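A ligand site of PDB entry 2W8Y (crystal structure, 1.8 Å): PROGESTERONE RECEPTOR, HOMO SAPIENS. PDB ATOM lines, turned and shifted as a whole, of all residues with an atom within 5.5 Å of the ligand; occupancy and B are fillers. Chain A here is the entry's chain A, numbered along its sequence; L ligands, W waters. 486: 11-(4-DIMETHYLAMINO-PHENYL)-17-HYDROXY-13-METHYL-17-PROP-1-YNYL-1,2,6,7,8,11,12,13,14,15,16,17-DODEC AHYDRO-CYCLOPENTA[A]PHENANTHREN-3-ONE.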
ATOM      1  N   LEU A  42     -24.744   5.575  19.909  1.00  0.00           N
ATOM      2  CA  LEU A  42     -24.271   5.524  21.282  1.00  0.00           C
ATOM      3  C   LEU A  42     -22.751   5.524  21.329  1.00  0.00           C
ATOM      4  O   LEU A  42     -22.162   6.200  22.161  1.00  0.00           O
ATOM      5  CB  LEU A  42     -24.863   4.314  22.021  1.00  0.00           C
ATOM      6  CG  LEU A  42     -26.341   4.428  22.435  1.00  0.00           C
ATOM      7  CD1 LEU A  42     -26.803   3.140  23.126  1.00  0.00           C
ATOM      8  CD2 LEU A  42     -26.610   5.616  23.321  1.00  0.00           C
ATOM      9  N   LEU A  45     -21.469   8.943  20.457  1.00  0.00           N
ATOM     10  CA  LEU A  45     -21.683   9.790  21.627  1.00  0.00           C
ATOM     11  C   LEU A  45     -20.597   9.557  22.690  1.00  0.00           C
ATOM     12  O   LEU A  45     -20.096  10.506  23.306  1.00  0.00           O
ATOM     13  CB  LEU A  45     -23.090   9.598  22.219  1.00  0.00           C
ATOM     14  CG  LEU A  45     -24.206  10.351  21.480  1.00  0.00           C
ATOM     15  CD1 LEU A  45     -25.575   9.880  21.941  1.00  0.00           C
ATOM     16  CD2 LEU A  45     -24.073  11.854  21.703  1.00  0.00           C
ATOM     17  N   ASN A  46     -20.215   8.286  22.873  1.00  0.00           N
ATOM     18  CA  ASN A  46     -19.155   7.919  23.809  1.00  0.00           C
ATOM     19  C   ASN A  46     -17.790   8.412  23.359  1.00  0.00           C
ATOM     20  O   ASN A  46     -16.979   8.843  24.175  1.00  0.00           O
ATOM     21  CB  ASN A  46     -19.118   6.403  24.031  1.00  0.00           C
ATOM     22  CG  ASN A  46     -20.338   5.870  24.808  1.00  0.00           C
ATOM     23  OD1 ASN A  46     -21.133   6.644  25.351  1.00  0.00           O
ATOM     24  ND2 ASN A  46     -20.467   4.560  24.871  1.00  0.00           N
ATOM     25  N   LEU A  48     -17.308  11.078  21.413  1.00  0.00           N
ATOM     26  CA  LEU A  48     -17.397  12.514  21.599  1.00  0.00           C
ATOM     27  C   LEU A  48     -17.243  12.892  23.070  1.00  0.00           C
ATOM     28  O   LEU A  48     -16.603  13.895  23.392  1.00  0.00           O
ATOM     29  CB  LEU A  48     -18.752  13.027  21.092  1.00  0.00           C
ATOM     30  CG  LEU A  48     -19.025  14.508  21.245  1.00  0.00           C
ATOM     31  CD1 LEU A  48     -18.031  15.315  20.453  1.00  0.00           C
ATOM     32  CD2 LEU A  48     -20.467  14.813  20.795  1.00  0.00           C
ATOM     33  N   GLY A  49     -17.872  12.109  23.940  1.00  0.00           N
ATOM     34  CA  GLY A  49     -17.757  12.297  25.377  1.00  0.00           C
ATOM     35  C   GLY A  49     -16.323  12.233  25.870  1.00  0.00           C
ATOM     36  O   GLY A  49     -15.905  13.060  26.676  1.00  0.00           O
ATOM     37  N   GLU A  50     -15.574  11.264  25.367  1.00  0.00           N
ATOM     38  CA  GLU A  50     -14.155  11.122  25.699  1.00  0.00           C
ATOM     39  C   GLU A  50     -13.366  12.374  25.308  1.00  0.00           C
ATOM     40  O   GLU A  50     -12.615  12.929  26.117  1.00  0.00           O
ATOM     41  CB  GLU A  50     -13.577   9.898  24.954  1.00  0.00           C
ATOM     42  CG  GLU A  50     -12.119   9.604  25.197  1.00  0.00           C
ATOM     43  CD  GLU A  50     -11.871   8.971  26.542  1.00  0.00           C
ATOM     44  OE1 GLU A  50     -12.807   8.961  27.376  1.00  0.00           O
ATOM     45  OE2 GLU A  50     -10.736   8.475  26.778  1.00  0.00           O
ATOM     46  N   GLN A  52     -14.654  15.389  24.694  1.00  0.00           N
ATOM     47  CA  GLN A  52     -15.100  16.501  25.514  1.00  0.00           C
ATOM     48  C   GLN A  52     -14.518  16.460  26.926  1.00  0.00           C
ATOM     49  O   GLN A  52     -14.230  17.511  27.494  1.00  0.00           O
ATOM     50  CB  GLN A  52     -16.617  16.608  25.558  1.00  0.00           C
ATOM     51  CG  GLN A  52     -17.182  17.131  24.247  1.00  0.00           C
ATOM     52  CD  GLN A  52     -18.676  17.300  24.286  1.00  0.00           C
ATOM     53  OE1 GLN A  52     -19.282  17.282  25.359  1.00  0.00           O
ATOM     54  NE2 GLN A  52     -19.285  17.451  23.105  1.00  0.00           N
ATOM     55  N   LEU A  53     -14.320  15.257  27.463  1.00  0.00           N
ATOM     56  CA  LEU A  53     -13.703  15.113  28.786  1.00  0.00           C
ATOM     57  C   LEU A  53     -12.262  15.605  28.779  1.00  0.00           C
ATOM     58  O   LEU A  53     -11.851  16.327  29.688  1.00  0.00           O
ATOM     59  CB  LEU A  53     -13.784  13.670  29.297  1.00  0.00           C
ATOM     60  CG  LEU A  53     -13.324  13.408  30.733  1.00  0.00           C
ATOM     61  CD1 LEU A  53     -14.103  14.262  31.722  1.00  0.00           C
ATOM     62  CD2 LEU A  53     -13.441  11.922  31.078  1.00  0.00           C
ATOM     63  N   TRP A  82     -18.698  16.216  35.289  1.00  0.00           N
ATOM     64  CA  TRP A  82     -18.531  16.148  33.826  1.00  0.00           C
ATOM     65  C   TRP A  82     -19.860  16.055  33.076  1.00  0.00           C
ATOM     66  O   TRP A  82     -20.008  16.658  32.016  1.00  0.00           O
ATOM     67  CB  TRP A  82     -17.566  15.033  33.390  1.00  0.00           C
ATOM     68  CG  TRP A  82     -18.001  13.656  33.739  1.00  0.00           C
ATOM     69  CD1 TRP A  82     -17.627  12.950  34.834  1.00  0.00           C
ATOM     70  CD2 TRP A  82     -18.904  12.819  33.002  1.00  0.00           C
ATOM     71  NE1 TRP A  82     -18.235  11.728  34.831  1.00  0.00           N
ATOM     72  CE2 TRP A  82     -19.018  11.619  33.715  1.00  0.00           C
ATOM     73  CE3 TRP A  82     -19.612  12.968  31.800  1.00  0.00           C
ATOM     74  CZ2 TRP A  82     -19.820  10.560  33.282  1.00  0.00           C
ATOM     75  CZ3 TRP A  82     -20.404  11.929  31.376  1.00  0.00           C
ATOM     76  CH2 TRP A  82     -20.506  10.736  32.106  1.00  0.00           C
ATOM     77  N   MET A  83     -20.842  15.331  33.621  1.00  0.00           N
ATOM     78  CA  MET A  83     -22.117  15.165  32.941  1.00  0.00           C
ATOM     79  C   MET A  83     -22.831  16.504  32.847  1.00  0.00           C
ATOM     80  O   MET A  83     -23.359  16.878  31.792  1.00  0.00           O
ATOM     81  CB  MET A  83     -23.005  14.140  33.670  1.00  0.00           C
ATOM     82  CG  MET A  83     -24.312  13.848  32.935  1.00  0.00           C
ATOM     83  SD  MET A  83     -24.051  12.932  31.409  1.00  0.00           S
ATOM     84  CE  MET A  83     -23.783  11.294  32.083  1.00  0.00           C
ATOM     85  N   MET A  86     -21.121  18.721  30.312  1.00  0.00           N
ATOM     86  CA  MET A  86     -21.383  18.300  28.925  1.00  0.00           C
ATOM     87  C   MET A  86     -22.798  18.618  28.459  1.00  0.00           C
ATOM     88  O   MET A  86     -22.980  19.080  27.345  1.00  0.00           O
ATOM     89  CB  MET A  86     -21.068  16.838  28.722  1.00  0.00           C
ATOM     90  CG  MET A  86     -19.597  16.536  28.789  1.00  0.00           C
ATOM     91  SD  MET A  86     -19.264  14.824  28.419  1.00  0.00           S
ATOM     92  CE  MET A  86     -17.588  14.678  29.056  1.00  0.00           C
ATOM     93  N   VAL A  87     -23.792  18.392  29.314  1.00  0.00           N
ATOM     94  CA  VAL A  87     -25.181  18.680  28.915  1.00  0.00           C
ATOM     95  C   VAL A  87     -25.422  20.193  28.827  1.00  0.00           C
ATOM     96  O   VAL A  87     -26.153  20.650  27.957  1.00  0.00           O
ATOM     97  CB  VAL A  87     -26.237  17.983  29.832  1.00  0.00           C
ATOM     98  CG1 VAL A  87     -26.441  18.732  31.152  1.00  0.00           C
ATOM     99  CG2 VAL A  87     -27.582  17.849  29.085  1.00  0.00           C
ATOM    100  N   LEU A  90     -23.822  21.222  25.636  1.00  0.00           N
ATOM    101  CA  LEU A  90     -24.759  20.788  24.591  1.00  0.00           C
ATOM    102  C   LEU A  90     -25.912  21.781  24.421  1.00  0.00           C
ATOM    103  O   LEU A  90     -26.269  22.132  23.291  1.00  0.00           O
ATOM    104  CB  LEU A  90     -25.323  19.397  24.915  1.00  0.00           C
ATOM    105  CG  LEU A  90     -26.477  18.877  24.036  1.00  0.00           C
ATOM    106  CD1 LEU A  90     -26.015  18.659  22.604  1.00  0.00           C
ATOM    107  CD2 LEU A  90     -27.039  17.600  24.626  1.00  0.00           C
ATOM    108  N   ARG A  93     -24.480  25.101  22.682  1.00  0.00           N
ATOM    109  CA  ARG A  93     -24.231  24.937  21.253  1.00  0.00           C
ATOM    110  C   ARG A  93     -25.538  24.843  20.468  1.00  0.00           C
ATOM    111  O   ARG A  93     -25.627  25.371  19.365  1.00  0.00           O
ATOM    112  CB  ARG A  93     -23.389  23.681  20.995  1.00  0.00           C
ATOM    113  CG  ARG A  93     -21.975  23.739  21.533  1.00  0.00           C
ATOM    114  CD  ARG A  93     -21.166  22.540  21.027  1.00  0.00           C
ATOM    115  NE  ARG A  93     -21.735  21.270  21.475  1.00  0.00           N
ATOM    116  CZ  ARG A  93     -21.456  20.683  22.641  1.00  0.00           C
ATOM    117  NH1 ARG A  93     -20.615  21.226  23.502  1.00  0.00           N
ATOM    118  NH2 ARG A  93     -22.032  19.525  22.948  1.00  0.00           N
ATOM    119  N   PHE A 105     -24.767  18.154  19.327  1.00  0.00           N
ATOM    120  CA  PHE A 105     -23.695  17.445  20.055  1.00  0.00           C
ATOM    121  C   PHE A 105     -22.336  17.853  19.524  1.00  0.00           C
ATOM    122  O   PHE A 105     -21.410  18.165  20.295  1.00  0.00           O
ATOM    123  CB  PHE A 105     -23.865  15.931  19.931  1.00  0.00           C
ATOM    124  CG  PHE A 105     -25.050  15.395  20.671  1.00  0.00           C
ATOM    125  CD1 PHE A 105     -24.972  15.174  22.032  1.00  0.00           C
ATOM    126  CD2 PHE A 105     -26.241  15.098  20.014  1.00  0.00           C
ATOM    127  CE1 PHE A 105     -26.061  14.676  22.742  1.00  0.00           C
ATOM    128  CE2 PHE A 105     -27.345  14.601  20.717  1.00  0.00           C
ATOM    129  CZ  PHE A 105     -27.243  14.399  22.084  1.00  0.00           C
ATOM    130  N   PHE A 121     -33.502   6.385  21.647  1.00  0.00           N
ATOM    131  CA  PHE A 121     -33.532   7.019  22.962  1.00  0.00           C
ATOM    132  C   PHE A 121     -34.180   8.412  22.895  1.00  0.00           C
ATOM    133  O   PHE A 121     -33.592   9.397  23.360  1.00  0.00           O
ATOM    134  CB  PHE A 121     -32.138   7.100  23.576  1.00  0.00           C
ATOM    135  CG  PHE A 121     -31.077   7.605  22.626  1.00  0.00           C
ATOM    136  CD1 PHE A 121     -30.484   6.747  21.717  1.00  0.00           C
ATOM    137  CD2 PHE A 121     -30.690   8.924  22.654  1.00  0.00           C
ATOM    138  CE1 PHE A 121     -29.510   7.215  20.846  1.00  0.00           C
ATOM    139  CE2 PHE A 121     -29.714   9.391  21.794  1.00  0.00           C
ATOM    140  CZ  PHE A 121     -29.129   8.526  20.885  1.00  0.00           C
ATOM    141  N   LEU A 124     -34.808  10.308  26.265  1.00  0.00           N
ATOM    142  CA  LEU A 124     -33.560  10.905  26.737  1.00  0.00           C
ATOM    143  C   LEU A 124     -33.263  12.187  25.947  1.00  0.00           C
ATOM    144  O   LEU A 124     -32.894  13.199  26.539  1.00  0.00           O
ATOM    145  CB  LEU A 124     -32.378   9.930  26.656  1.00  0.00           C
ATOM    146  CG  LEU A 124     -31.138  10.382  27.446  1.00  0.00           C
ATOM    147  CD1 LEU A 124     -31.344  10.169  28.936  1.00  0.00           C
ATOM    148  CD2 LEU A 124     -29.870   9.669  27.011  1.00  0.00           C
ATOM    149  N   MET A 128     -32.833  15.992  27.455  1.00  0.00           N
ATOM    150  CA  MET A 128     -31.678  16.844  27.192  1.00  0.00           C
ATOM    151  C   MET A 128     -32.082  18.142  26.473  1.00  0.00           C
ATOM    152  O   MET A 128     -31.532  19.220  26.762  1.00  0.00           O
ATOM    153  CB  MET A 128     -30.618  16.083  26.391  1.00  0.00           C
ATOM    154  CG  MET A 128     -29.922  14.998  27.215  1.00  0.00           C
ATOM    155  SD  MET A 128     -28.565  14.157  26.363  1.00  0.00           S
ATOM    156  CE  MET A 128     -29.419  13.089  25.217  1.00  0.00           C
ATOM    157  N   LEU A 214     -29.585  11.263  33.480  1.00  0.00           N
ATOM    158  CA  LEU A 214     -28.498  11.010  32.533  1.00  0.00           C
ATOM    159  C   LEU A 214     -27.457  10.068  33.134  1.00  0.00           C
ATOM    160  O   LEU A 214     -26.963   9.174  32.458  1.00  0.00           O
ATOM    161  CB  LEU A 214     -27.815  12.324  32.103  1.00  0.00           C
ATOM    162  CG  LEU A 214     -28.687  13.420  31.478  1.00  0.00           C
ATOM    163  CD1 LEU A 214     -27.817  14.525  30.886  1.00  0.00           C
ATOM    164  CD2 LEU A 214     -29.615  12.887  30.431  1.00  0.00           C
ATOM    165  N   TYR A 217     -29.016   6.459  33.051  1.00  0.00           N
ATOM    166  CA  TYR A 217     -28.963   5.965  31.671  1.00  0.00           C
ATOM    167  C   TYR A 217     -27.533   5.542  31.316  1.00  0.00           C
ATOM    168  O   TYR A 217     -27.314   4.465  30.757  1.00  0.00           O
ATOM    169  CB  TYR A 217     -29.430   7.038  30.698  1.00  0.00           C
ATOM    170  CG  TYR A 217     -29.656   6.502  29.303  1.00  0.00           C
ATOM    171  CD1 TYR A 217     -28.611   6.364  28.406  1.00  0.00           C
ATOM    172  CD2 TYR A 217     -30.926   6.104  28.887  1.00  0.00           C
ATOM    173  CE1 TYR A 217     -28.806   5.848  27.127  1.00  0.00           C
ATOM    174  CE2 TYR A 217     -31.134   5.589  27.611  1.00  0.00           C
ATOM    175  CZ  TYR A 217     -30.075   5.472  26.742  1.00  0.00           C
ATOM    176  OH  TYR A 217     -30.258   4.963  25.481  1.00  0.00           O
ATOM    177  N   CYS A 218     -26.590   6.409  31.637  1.00  0.00           N
ATOM    178  CA  CYS A 218     -25.191   6.179  31.331  1.00  0.00           C
ATOM    179  C   CYS A 218     -24.689   4.919  32.030  1.00  0.00           C
ATOM    180  O   CYS A 218     -24.066   4.061  31.410  1.00  0.00           O
ATOM    181  CB  CYS A 218     -24.355   7.392  31.746  1.00  0.00           C
ATOM    182  SG  CYS A 218     -22.594   7.165  31.550  1.00  0.00           S
ATOM    183  N   THR A 221     -26.218   1.836  30.545  1.00  0.00           N
ATOM    184  CA  THR A 221     -25.624   1.563  29.239  1.00  0.00           C
ATOM    185  C   THR A 221     -24.226   0.954  29.380  1.00  0.00           C
ATOM    186  O   THR A 221     -23.859   0.073  28.608  1.00  0.00           O
ATOM    187  CB  THR A 221     -25.560   2.828  28.373  1.00  0.00           C
ATOM    188  OG1 THR A 221     -26.878   3.341  28.194  1.00  0.00           O
ATOM    189  CG2 THR A 221     -24.969   2.512  26.996  1.00  0.00           C
ATOM    190  N   PHE A 232     -17.168   2.020  25.230  1.00  0.00           N
ATOM    191  CA  PHE A 232     -16.877   3.102  26.164  1.00  0.00           C
ATOM    192  C   PHE A 232     -15.351   3.278  26.231  1.00  0.00           C
ATOM    193  O   PHE A 232     -14.652   2.346  26.606  1.00  0.00           O
ATOM    194  CB  PHE A 232     -17.448   2.787  27.555  1.00  0.00           C
ATOM    195  CG  PHE A 232     -18.926   3.076  27.674  1.00  0.00           C
ATOM    196  CD1 PHE A 232     -19.856   2.116  27.329  1.00  0.00           C
ATOM    197  CD2 PHE A 232     -19.368   4.313  28.126  1.00  0.00           C
ATOM    198  CE1 PHE A 232     -21.216   2.378  27.434  1.00  0.00           C
ATOM    199  CE2 PHE A 232     -20.734   4.582  28.232  1.00  0.00           C
ATOM    200  CZ  PHE A 232     -21.659   3.601  27.886  1.00  0.00           C
ATOM    201  N   PRO A 233     -14.844   4.467  25.856  1.00  0.00           N
ATOM    202  CA  PRO A 233     -13.406   4.748  25.891  1.00  0.00           C
ATOM    203  C   PRO A 233     -12.786   4.796  27.285  1.00  0.00           C
ATOM    204  O   PRO A 233     -13.507   4.769  28.290  1.00  0.00           O
ATOM    205  CB  PRO A 233     -13.296   6.125  25.220  1.00  0.00           C
ATOM    206  CG  PRO A 233     -14.476   6.223  24.369  1.00  0.00           C
ATOM    207  CD  PRO A 233     -15.567   5.526  25.120  1.00  0.00           C
ATOM    208  N   MET A 235     -11.039   7.092  29.407  1.00  0.00           N
ATOM    209  CA  MET A 235     -11.303   8.111  30.434  1.00  0.00           C
ATOM    210  C   MET A 235     -12.773   8.119  30.877  1.00  0.00           C
ATOM    211  O   MET A 235     -13.063   8.433  32.029  1.00  0.00           O
ATOM    212  CB  MET A 235     -10.890   9.517  29.967  1.00  0.00           C
ATOM    213  CG  MET A 235      -9.406   9.651  29.624  1.00  0.00           C
ATOM    214  SD  MET A 235      -8.313   9.193  30.992  1.00  0.00           S
ATOM    215  CE  MET A 235      -8.687  10.488  32.185  1.00  0.00           C
ATOM    216  N   MET A 236     -13.668   7.770  29.946  1.00  0.00           N
ATOM    217  CA  MET A 236     -15.084   7.604  30.275  1.00  0.00           C
ATOM    218  C   MET A 236     -15.296   6.468  31.263  1.00  0.00           C
ATOM    219  O   MET A 236     -15.953   6.643  32.286  1.00  0.00           O
ATOM    220  N   SER A 237     -14.705   5.310  30.955  1.00  0.00           N
ATOM    221  CA  SER A 237     -14.815   4.117  31.789  1.00  0.00           C
ATOM    222  C   SER A 237     -14.316   4.335  33.219  1.00  0.00           C
ATOM    223  O   SER A 237     -14.873   3.754  34.147  1.00  0.00           O
ATOM    224  CB  SER A 237     -14.060   2.962  31.151  1.00  0.00           C
ATOM    225  OG  SER A 237     -14.522   2.757  29.826  1.00  0.00           O
ATOM    226  N   VAL A 239     -14.007   7.474  34.841  1.00  0.00           N
ATOM    227  CA  VAL A 239     -14.831   8.477  35.533  1.00  0.00           C
ATOM    228  C   VAL A 239     -16.147   7.847  36.014  1.00  0.00           C
ATOM    229  O   VAL A 239     -16.646   8.192  37.087  1.00  0.00           O
ATOM    230  CB  VAL A 239     -15.107   9.760  34.696  1.00  0.00           C
ATOM    231  CG1 VAL A 239     -13.835  10.600  34.552  1.00  0.00           C
ATOM    232  CG2 VAL A 239     -15.713   9.421  33.339  1.00  0.00           C
HETATM  233  O30 486 L   1     -21.813  16.830  23.945  1.00  0.00           O
HETATM  234  C2  486 L   1     -22.002  15.839  24.623  1.00  0.00           C
HETATM  235  C1  486 L   1     -21.126  14.652  24.368  1.00  0.00           C
HETATM  236  C3  486 L   1     -23.019  15.841  25.585  1.00  0.00           C
HETATM  237  C4  486 L   1     -23.343  14.730  26.270  1.00  0.00           C
HETATM  238  C7  486 L   1     -24.370  14.847  27.368  1.00  0.00           C
HETATM  239  C5  486 L   1     -22.722  13.407  25.975  1.00  0.00           C
HETATM  240  C6  486 L   1     -21.648  13.323  24.919  1.00  0.00           C
HETATM  241  C10 486 L   1     -23.148  12.272  26.589  1.00  0.00           C
HETATM  242  C14 486 L   1     -22.524  10.913  26.211  1.00  0.00           C
HETATM  243  C18 486 L   1     -21.201  10.666  26.951  1.00  0.00           C
HETATM  244  C22 486 L   1     -20.613  11.576  27.824  1.00  0.00           C
HETATM  245  C23 486 L   1     -19.388  11.319  28.441  1.00  0.00           C
HETATM  246  C24 486 L   1     -18.704  10.121  28.206  1.00  0.00           C
HETATM  247  N27 486 L   1     -17.465   9.863  28.819  1.00  0.00           N
HETATM  248  C29 486 L   1     -17.026  10.521  30.059  1.00  0.00           C
HETATM  249  C28 486 L   1     -16.432   9.167  28.045  1.00  0.00           C
HETATM  250  C25 486 L   1     -19.266   9.209  27.317  1.00  0.00           C
HETATM  251  C26 486 L   1     -20.488   9.494  26.710  1.00  0.00           C
HETATM  252  C13 486 L   1     -23.528   9.726  26.310  1.00  0.00           C
HETATM  253  C12 486 L   1     -24.352   9.777  27.570  1.00  0.00           C
HETATM  254  C19 486 L   1     -23.439   9.711  28.802  1.00  0.00           C
HETATM  255  C17 486 L   1     -25.500   8.754  27.698  1.00  0.00           C
HETATM  256  C31 486 L   1     -26.289   8.581  26.461  1.00  0.00           C
HETATM  257  C30 486 L   1     -26.966   8.454  25.516  1.00  0.00           C
HETATM  258  C32 486 L   1     -27.868   8.287  24.363  1.00  0.00           C
HETATM  259  O3  486 L   1     -25.063   7.496  28.146  1.00  0.00           O
HETATM  260  C16 486 L   1     -26.414   9.396  28.755  1.00  0.00           C
HETATM  261  C15 486 L   1     -26.138  10.918  28.684  1.00  0.00           C
HETATM  262  C11 486 L   1     -25.151  11.100  27.524  1.00  0.00           C
HETATM  263  C9  486 L   1     -24.248  12.322  27.630  1.00  0.00           C
HETATM  264  C8  486 L   1     -25.137  13.542  27.489  1.00  0.00           C
HETATM  265  O   HOH W   1     -23.718   5.925  26.008  1.00  0.00           O
HETATM  266  O   HOH W   2     -20.734  19.243  25.734  1.00  0.00           O
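NE2 of Gln 52 sits close to NH2 of Arg 93 (3.4 Å). The guanidinium group (NH2) of Arg 93 is in hydrogen-bond range of the backbone carbonyl oxygen (O) of Phe 105 (3.0 Å). The backbone NH (N) of Met 236 sits at hydrogen-bond distance from the side-chain carboxylate (OE1) of Glu 50 (3.0 Å). OD1 of Asn 46 lies close to O of Leu 42, 3.4 Å away. The backbone NH (N) of Met 235 lies within hydrogen-bond range of the side-chain carboxylate (OE2) of Glu 50, 3.0 Å away. O of Tyr 217 lies within hydrogen-bond range of OG1 of Thr 221 (2.8 Å).
Water W1 bridges the side-chain amide oxygen of Asn 46 and an oxygen (O3) of the ligand.
The side-chain amide nitrogen of Gln 52 lies within hydrogen-bond range of an oxygen (O30) of the ligand (2.7 Å). The guanidinium group (NH2) of Arg 93 lies within hydrogen-bond range of an oxygen (O30) of the ligand (2.9 Å).
Residues that only touch the ligand: Leu 42, Leu 45, Asn 46, Leu 48, Gly 49, Glu 50, Leu 53, Trp 82, Met 83, Met 86, Phe 105, Phe 121, Leu 124, Met 128, Leu 214, Tyr 217, Cys 218, Met 236 and Val 239. Hydrophobic or aromatic side chains that line the ligand: Leu 42, Leu 45, Leu 48, Leu 53, Trp 82, Met 83, Met 86, Phe 105, Phe 121, Leu 124, Met 128, Tyr 217 and Val 239. Within 4 Å of the ligand: Leu 42, Leu 45, Asn 46, Leu 48, Gly 49, Glu 50, Gln 52, Leu 53, Trp 82, Met 83, Met 86, Arg 93, Phe 105, Phe 121, Leu 124, Met 128, Leu 214, Tyr 217, Cys 218, Met 236 and Val 239. Along chain A the residues within 4 Å of the ligand span positions 42 to 239.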
